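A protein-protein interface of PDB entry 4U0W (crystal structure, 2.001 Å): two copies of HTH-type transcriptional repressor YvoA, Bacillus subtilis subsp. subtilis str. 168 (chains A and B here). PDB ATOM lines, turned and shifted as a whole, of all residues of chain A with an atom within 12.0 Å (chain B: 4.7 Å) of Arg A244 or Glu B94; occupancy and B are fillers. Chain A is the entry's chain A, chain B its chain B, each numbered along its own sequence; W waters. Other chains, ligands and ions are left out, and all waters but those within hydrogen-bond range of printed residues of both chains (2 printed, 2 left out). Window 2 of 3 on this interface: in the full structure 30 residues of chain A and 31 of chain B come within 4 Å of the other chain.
The backbone NH (N) of Arg A244 is in hydrogen-bond range of the backbone carbonyl oxygen (O) of Ser B182 (2.7 Å).
O of Asp A243 lies within hydrogen-bond range of N of Leu B89, at 2.9 Å.
The guanidinium group (NH2) of Arg A244 is in salt-bridge range of the side-chain carboxylate (OE2) of Glu B94 (2.6 Å).
The guanidinium group (NH1) of Arg A244 sits at hydrogen-bond distance from the backbone carbonyl oxygen (O) of Leu B89, 3.0 Å away.
OG1 of Thr B90 sits at hydrogen-bond distance from OD1 of Asp B95.
N of Ser B91 sits at hydrogen-bond distance from OE1 of Glu B94, at 2.8 Å.
The backbone NH (N) of Ile B181 sits at hydrogen-bond distance from the side-chain carboxylate (OE2) of Glu B174, 2.9 Å away.
Among the printed residues, merely in contact across the chains: Arg A244 with Ile B181 (3.3 Å), Asp A243 with Ser B182 (3.4 Å), Met A242 with Leu B89 (3.8 Å), Arg A244 with Thr B90 (3.9 Å) and Met A242 with Ser B182 (3.999 Å).
His A240 touches none of the printed residues of chain B.
Tyr A241 touches none of the printed residues of chain B.
Printed residues of chain B within 4 Å of Met A242: Leu B89 and Ser B182.
Printed residues of chain B within 4 Å of Asp A243: Leu B89 (2.9 Å) and Ser B182 (3.4 Å).
Printed residues of chain B within 4 Å of Arg A244: Leu B89, Thr B90, Glu B94, Ile B181 and Ser B182.
Printed residues of chain A within 4 Å of Leu B89: Met A242 (3.8 Å), Asp A243 (2.9 Å) and Arg A244 (3.0 Å).
Of chain A, only Arg A244 comes within 4 Å of Glu B94.
No residue of chain A comes within 4 Å of Met B96.
No residue of chain A comes within 4 Å of Lys B97.
No residue of chain A comes within 4 Å of Ser B98.
Printed residues of chain A within 4 Å of Ser B182: Met A242, Asp A243 and Arg A244.
Hydrophobic or aromatic side chains of chain A that line the printed part of chain B: Met A242.
Printed residues of chain B that touch a printed residue of chain A: Leu B89, Thr B90, Glu B94, Ile B181 and Ser B182.
Hydrophobic or aromatic side chains of chain B that line the printed part of chain A: Leu B89 and Ile B181.
Along chain B the printed residues that touch a printed residue of chain A span positions 89 to 182.
Among the printed residues, 9 pairs touch across the chains.
Among the printed residues, Asp or Glu carboxylates within 4 Å of a Lys or Arg side-chain nitrogen of the other chain: Arg A244 with Glu B94 (2.6 Å).
No position is printed for both chains.
Of the 9 pairs that touch across the chains among the printed residues, none has its exchanged pair printed and touching as well.
Water W1 bridges the side-chain hydroxyl of Thr B90 (2.7 Å) and the side-chain sulfur of Met A242 (3.6 Å).
Water W2 lies within hydrogen-bond range of the backbone NH of Leu A245 and the backbone carbonyl oxygen of Leu B89.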
ATOM      1  N   GLN A  87     -40.720 -14.528  -0.752  1.00  0.00           N
ATOM      2  CA  GLN A  87     -41.222 -13.165  -0.949  1.00  0.00           C
ATOM      3  C   GLN A  87     -42.638 -13.077  -1.542  1.00  0.00           C
ATOM      4  O   GLN A  87     -43.257 -12.017  -1.509  1.00  0.00           O
ATOM      5  CB  GLN A  87     -40.234 -12.389  -1.815  1.00  0.00           C
ATOM      6  CG  GLN A  87     -39.000 -11.943  -1.030  1.00  0.00           C
ATOM      7  CD  GLN A  87     -37.788 -11.730  -1.915  1.00  0.00           C
ATOM      8  OE1 GLN A  87     -37.378 -12.633  -2.651  1.00  0.00           O
ATOM      9  NE2 GLN A  87     -37.212 -10.537  -1.857  1.00  0.00           N
ATOM     10  N   HIS A 240     -34.997 -16.553  -1.100  1.00  0.00           N
ATOM     11  CA  HIS A 240     -35.406 -15.163  -1.213  1.00  0.00           C
ATOM     12  C   HIS A 240     -34.278 -14.367  -1.856  1.00  0.00           C
ATOM     13  O   HIS A 240     -33.156 -14.864  -1.994  1.00  0.00           O
ATOM     14  CB  HIS A 240     -35.753 -14.594   0.154  1.00  0.00           C
ATOM     15  CG  HIS A 240     -34.564 -14.444   1.042  1.00  0.00           C
ATOM     16  ND1 HIS A 240     -33.926 -13.237   1.235  1.00  0.00           N
ATOM     17  CD2 HIS A 240     -33.859 -15.361   1.743  1.00  0.00           C
ATOM     18  CE1 HIS A 240     -32.892 -13.414   2.039  1.00  0.00           C
ATOM     19  NE2 HIS A 240     -32.831 -14.695   2.363  1.00  0.00           N
ATOM     20  N   TYR A 241     -34.578 -13.137  -2.246  1.00  0.00           N
ATOM     21  CA  TYR A 241     -33.610 -12.272  -2.904  1.00  0.00           C
ATOM     22  C   TYR A 241     -33.464 -10.976  -2.119  1.00  0.00           C
ATOM     23  O   TYR A 241     -34.373 -10.575  -1.389  1.00  0.00           O
ATOM     24  CB  TYR A 241     -34.035 -12.007  -4.351  1.00  0.00           C
ATOM     25  CG  TYR A 241     -34.060 -13.267  -5.171  1.00  0.00           C
ATOM     26  CD1 TYR A 241     -35.156 -14.123  -5.136  1.00  0.00           C
ATOM     27  CD2 TYR A 241     -32.968 -13.627  -5.960  1.00  0.00           C
ATOM     28  CE1 TYR A 241     -35.168 -15.302  -5.877  1.00  0.00           C
ATOM     29  CE2 TYR A 241     -32.971 -14.800  -6.696  1.00  0.00           C
ATOM     30  CZ  TYR A 241     -34.069 -15.632  -6.652  1.00  0.00           C
ATOM     31  OH  TYR A 241     -34.063 -16.796  -7.382  1.00  0.00           O
ATOM     32  N   MET A 242     -32.310 -10.334  -2.252  1.00  0.00           N
ATOM     33  CA  MET A 242     -32.053  -9.070  -1.571  1.00  0.00           C
ATOM     34  C   MET A 242     -31.475  -8.032  -2.518  1.00  0.00           C
ATOM     35  O   MET A 242     -30.668  -8.356  -3.383  1.00  0.00           O
ATOM     36  CB  MET A 242     -31.100  -9.270  -0.392  1.00  0.00           C
ATOM     37  CG  MET A 242     -31.655 -10.144   0.704  1.00  0.00           C
ATOM     38  SD  MET A 242     -30.518 -10.412   2.092  1.00  0.00           S
ATOM     39  CE  MET A 242     -29.208 -11.294   1.246  1.00  0.00           C
ATOM     40  N   ASP A 243     -31.894  -6.781  -2.353  1.00  0.00           N
ATOM     41  CA  ASP A 243     -31.288  -5.682  -3.085  1.00  0.00           C
ATOM     42  C   ASP A 243     -30.526  -4.797  -2.106  1.00  0.00           C
ATOM     43  O   ASP A 243     -30.820  -4.781  -0.917  1.00  0.00           O
ATOM     44  CB  ASP A 243     -32.340  -4.868  -3.840  1.00  0.00           C
ATOM     45  CG  ASP A 243     -33.094  -5.694  -4.868  1.00  0.00           C
ATOM     46  OD1 ASP A 243     -32.475  -6.570  -5.510  1.00  0.00           O
ATOM     47  OD2 ASP A 243     -34.312  -5.466  -5.038  1.00  0.00           O
ATOM     48  N   ARG A 244     -29.524  -4.092  -2.618  1.00  0.00           N
ATOM     49  CA  ARG A 244     -28.740  -3.157  -1.828  1.00  0.00           C
ATOM     50  C   ARG A 244     -29.524  -1.861  -1.691  1.00  0.00           C
ATOM     51  O   ARG A 244     -30.045  -1.363  -2.688  1.00  0.00           O
ATOM     52  CB  ARG A 244     -27.386  -2.911  -2.499  1.00  0.00           C
ATOM     53  CG  ARG A 244     -26.466  -1.967  -1.762  1.00  0.00           C
ATOM     54  CD  ARG A 244     -26.070  -2.528  -0.421  1.00  0.00           C
ATOM     55  NE  ARG A 244     -24.900  -1.843   0.109  1.00  0.00           N
ATOM     56  CZ  ARG A 244     -24.457  -1.988   1.353  1.00  0.00           C
ATOM     57  NH1 ARG A 244     -25.098  -2.790   2.196  1.00  0.00           N
ATOM     58  NH2 ARG A 244     -23.382  -1.322   1.755  1.00  0.00           N
ATOM     59  N   LEU A 245     -29.586  -1.339  -0.462  1.00  0.00           N
ATOM     60  CA  LEU A 245     -30.427  -0.200  -0.035  1.00  0.00           C
ATOM     61  C   LEU A 245     -31.851  -0.651   0.276  1.00  0.00           C
ATOM     62  O   LEU A 245     -32.085  -1.797   0.664  1.00  0.00           O
ATOM     63  CB  LEU A 245     -30.474   0.929  -1.078  1.00  0.00           C
ATOM     64  CG  LEU A 245     -29.376   1.994  -1.125  1.00  0.00           C
ATOM     65  CD1 LEU A 245     -28.027   1.401  -1.523  1.00  0.00           C
ATOM     66  CD2 LEU A 245     -29.782   3.123  -2.070  1.00  0.00           C
ATOM     67  N   LEU B  89     -29.813  -6.227   1.446  1.00  0.00           N
ATOM     68  CA  LEU B  89     -28.507  -6.866   1.316  1.00  0.00           C
ATOM     69  C   LEU B  89     -27.454  -6.081   2.103  1.00  0.00           C
ATOM     70  O   LEU B  89     -27.134  -4.934   1.780  1.00  0.00           O
ATOM     71  CB  LEU B  89     -28.106  -6.978  -0.162  1.00  0.00           C
ATOM     72  CG  LEU B  89     -26.689  -7.458  -0.485  1.00  0.00           C
ATOM     73  CD1 LEU B  89     -26.397  -8.816   0.171  1.00  0.00           C
ATOM     74  CD2 LEU B  89     -26.508  -7.535  -2.013  1.00  0.00           C
ATOM     75  N   THR B  90     -26.916  -6.716   3.137  1.00  0.00           N
ATOM     76  CA  THR B  90     -25.974  -6.078   4.042  1.00  0.00           C
ATOM     77  C   THR B  90     -24.859  -7.031   4.451  1.00  0.00           C
ATOM     78  O   THR B  90     -24.983  -8.242   4.309  1.00  0.00           O
ATOM     79  CB  THR B  90     -26.672  -5.600   5.335  1.00  0.00           C
ATOM     80  OG1 THR B  90     -27.264  -6.734   5.977  1.00  0.00           O
ATOM     81  CG2 THR B  90     -27.747  -4.560   5.035  1.00  0.00           C
ATOM     82  N   SER B  91     -23.783  -6.474   4.994  1.00  0.00           N
ATOM     83  CA  SER B  91     -22.718  -7.289   5.551  1.00  0.00           C
ATOM     84  C   SER B  91     -22.965  -7.549   7.031  1.00  0.00           C
ATOM     85  O   SER B  91     -23.752  -6.840   7.683  1.00  0.00           O
ATOM     86  CB  SER B  91     -21.364  -6.604   5.361  1.00  0.00           C
ATOM     87  OG  SER B  91     -21.267  -5.490   6.233  1.00  0.00           O
ATOM     88  N   PHE B  92     -22.288  -8.566   7.550  1.00  0.00           N
ATOM     89  CA  PHE B  92     -22.225  -8.803   8.982  1.00  0.00           C
ATOM     90  C   PHE B  92     -21.796  -7.534   9.723  1.00  0.00           C
ATOM     91  O   PHE B  92     -22.414  -7.147  10.723  1.00  0.00           O
ATOM     92  CB  PHE B  92     -21.256  -9.943   9.291  1.00  0.00           C
ATOM     93  CG  PHE B  92     -21.230 -10.340  10.743  1.00  0.00           C
ATOM     94  CD1 PHE B  92     -22.166 -11.228  11.248  1.00  0.00           C
ATOM     95  CD2 PHE B  92     -20.254  -9.842  11.594  1.00  0.00           C
ATOM     96  CE1 PHE B  92     -22.151 -11.604  12.581  1.00  0.00           C
ATOM     97  CE2 PHE B  92     -20.230 -10.214  12.940  1.00  0.00           C
ATOM     98  CZ  PHE B  92     -21.183 -11.093  13.429  1.00  0.00           C
ATOM     99  N   THR B  93     -20.743  -6.892   9.220  1.00  0.00           N
ATOM    100  CA  THR B  93     -20.195  -5.703   9.851  1.00  0.00           C
ATOM    101  C   THR B  93     -21.260  -4.612   9.949  1.00  0.00           C
ATOM    102  O   THR B  93     -21.416  -3.993  10.996  1.00  0.00           O
ATOM    103  CB  THR B  93     -18.963  -5.172   9.091  1.00  0.00           C
ATOM    104  OG1 THR B  93     -17.852  -6.038   9.336  1.00  0.00           O
ATOM    105  CG2 THR B  93     -18.595  -3.787   9.578  1.00  0.00           C
ATOM    106  N   GLU B  94     -22.006  -4.412   8.864  1.00  0.00           N
ATOM    107  CA  GLU B  94     -23.131  -3.476   8.848  1.00  0.00           C
ATOM    108  C   GLU B  94     -24.235  -3.866   9.830  1.00  0.00           C
ATOM    109  O   GLU B  94     -24.797  -2.999  10.528  1.00  0.00           O
ATOM    110  CB  GLU B  94     -23.714  -3.373   7.436  1.00  0.00           C
ATOM    111  CG  GLU B  94     -22.863  -2.565   6.483  1.00  0.00           C
ATOM    112  CD  GLU B  94     -23.283  -2.717   5.022  1.00  0.00           C
ATOM    113  OE1 GLU B  94     -24.035  -3.658   4.684  1.00  0.00           O
ATOM    114  OE2 GLU B  94     -22.856  -1.878   4.207  1.00  0.00           O
ATOM    115  N   ASP B  95     -24.556  -5.159   9.875  1.00  0.00           N
ATOM    116  CA  ASP B  95     -25.630  -5.642  10.735  1.00  0.00           C
ATOM    117  C   ASP B  95     -25.311  -5.385  12.202  1.00  0.00           C
ATOM    118  O   ASP B  95     -26.178  -4.962  12.970  1.00  0.00           O
ATOM    119  CB  ASP B  95     -25.886  -7.135  10.531  1.00  0.00           C
ATOM    120  CG  ASP B  95     -26.380  -7.469   9.128  1.00  0.00           C
ATOM    121  OD1 ASP B  95     -26.846  -6.562   8.408  1.00  0.00           O
ATOM    122  OD2 ASP B  95     -26.323  -8.658   8.757  1.00  0.00           O
ATOM    123  N   MET B  96     -24.067  -5.639  12.593  1.00  0.00           N
ATOM    124  CA  MET B  96     -23.691  -5.538  13.999  1.00  0.00           C
ATOM    125  C   MET B  96     -23.615  -4.075  14.451  1.00  0.00           C
ATOM    126  O   MET B  96     -24.051  -3.729  15.552  1.00  0.00           O
ATOM    127  CB  MET B  96     -22.368  -6.263  14.248  1.00  0.00           C
ATOM    128  CG  MET B  96     -22.519  -7.785  14.236  1.00  0.00           C
ATOM    129  SD  MET B  96     -23.794  -8.318  15.397  1.00  0.00           S
ATOM    130  CE  MET B  96     -24.219  -9.960  14.844  1.00  0.00           C
ATOM    131  N   LYS B  97     -23.086  -3.217  13.586  1.00  0.00           N
ATOM    132  CA  LYS B  97     -23.023  -1.795  13.882  1.00  0.00           C
ATOM    133  C   LYS B  97     -24.426  -1.237  14.076  1.00  0.00           C
ATOM    134  O   LYS B  97     -24.678  -0.486  15.013  1.00  0.00           O
ATOM    135  CB  LYS B  97     -22.293  -1.040  12.768  1.00  0.00           C
ATOM    136  CG  LYS B  97     -20.793  -1.279  12.756  1.00  0.00           C
ATOM    137  CD  LYS B  97     -20.116  -0.458  11.680  1.00  0.00           C
ATOM    138  CE  LYS B  97     -18.614  -0.652  11.722  1.00  0.00           C
ATOM    139  NZ  LYS B  97     -17.932   0.125  10.657  1.00  0.00           N
ATOM    140  N   SER B  98     -25.341  -1.630  13.196  1.00  0.00           N
ATOM    141  CA  SER B  98     -26.727  -1.192  13.275  1.00  0.00           C
ATOM    142  C   SER B  98     -27.381  -1.537  14.611  1.00  0.00           C
ATOM    143  O   SER B  98     -28.270  -0.828  15.062  1.00  0.00           O
ATOM    144  CB  SER B  98     -27.545  -1.811  12.148  1.00  0.00           C
ATOM    145  OG  SER B  98     -27.933  -3.128  12.487  1.00  0.00           O
ATOM    146  N   GLU B 174     -16.174  -3.605  -2.434  1.00  0.00           N
ATOM    147  CA  GLU B 174     -16.608  -2.375  -3.098  1.00  0.00           C
ATOM    148  C   GLU B 174     -15.410  -1.484  -3.451  1.00  0.00           C
ATOM    149  O   GLU B 174     -15.318  -0.948  -4.564  1.00  0.00           O
ATOM    150  CB  GLU B 174     -17.613  -1.623  -2.216  1.00  0.00           C
ATOM    151  CG  GLU B 174     -18.933  -2.374  -2.078  1.00  0.00           C
ATOM    152  CD  GLU B 174     -20.081  -1.504  -1.581  1.00  0.00           C
ATOM    153  OE1 GLU B 174     -19.876  -0.712  -0.639  1.00  0.00           O
ATOM    154  OE2 GLU B 174     -21.195  -1.625  -2.137  1.00  0.00           O
ATOM    155  N   ILE B 181     -21.876  -3.362  -4.325  1.00  0.00           N
ATOM    156  CA  ILE B 181     -22.668  -4.587  -4.226  1.00  0.00           C
ATOM    157  C   ILE B 181     -24.118  -4.220  -4.500  1.00  0.00           C
ATOM    158  O   ILE B 181     -24.561  -3.122  -4.153  1.00  0.00           O
ATOM    159  CB  ILE B 181     -22.532  -5.260  -2.833  1.00  0.00           C
ATOM    160  CG1 ILE B 181     -23.066  -4.333  -1.735  1.00  0.00           C
ATOM    161  CG2 ILE B 181     -21.069  -5.637  -2.561  1.00  0.00           C
ATOM    162  CD1 ILE B 181     -23.067  -4.926  -0.341  1.00  0.00           C
ATOM    163  N   SER B 182     -24.869  -5.114  -5.133  1.00  0.00           N
ATOM    164  CA  SER B 182     -26.227  -4.729  -5.507  1.00  0.00           C
ATOM    165  C   SER B 182     -27.308  -5.743  -5.185  1.00  0.00           C
ATOM    166  O   SER B 182     -28.385  -5.365  -4.736  1.00  0.00           O
ATOM    167  CB  SER B 182     -26.288  -4.394  -7.001  1.00  0.00           C
ATOM    168  OG  SER B 182     -25.781  -5.447  -7.787  1.00  0.00           O
HETATM  169  O   HOH W   1     -28.524  -8.563   4.462  1.00  0.00           O
HETATM  170  O   HOH W   2     -28.928  -2.711   1.947  1.00  0.00           O
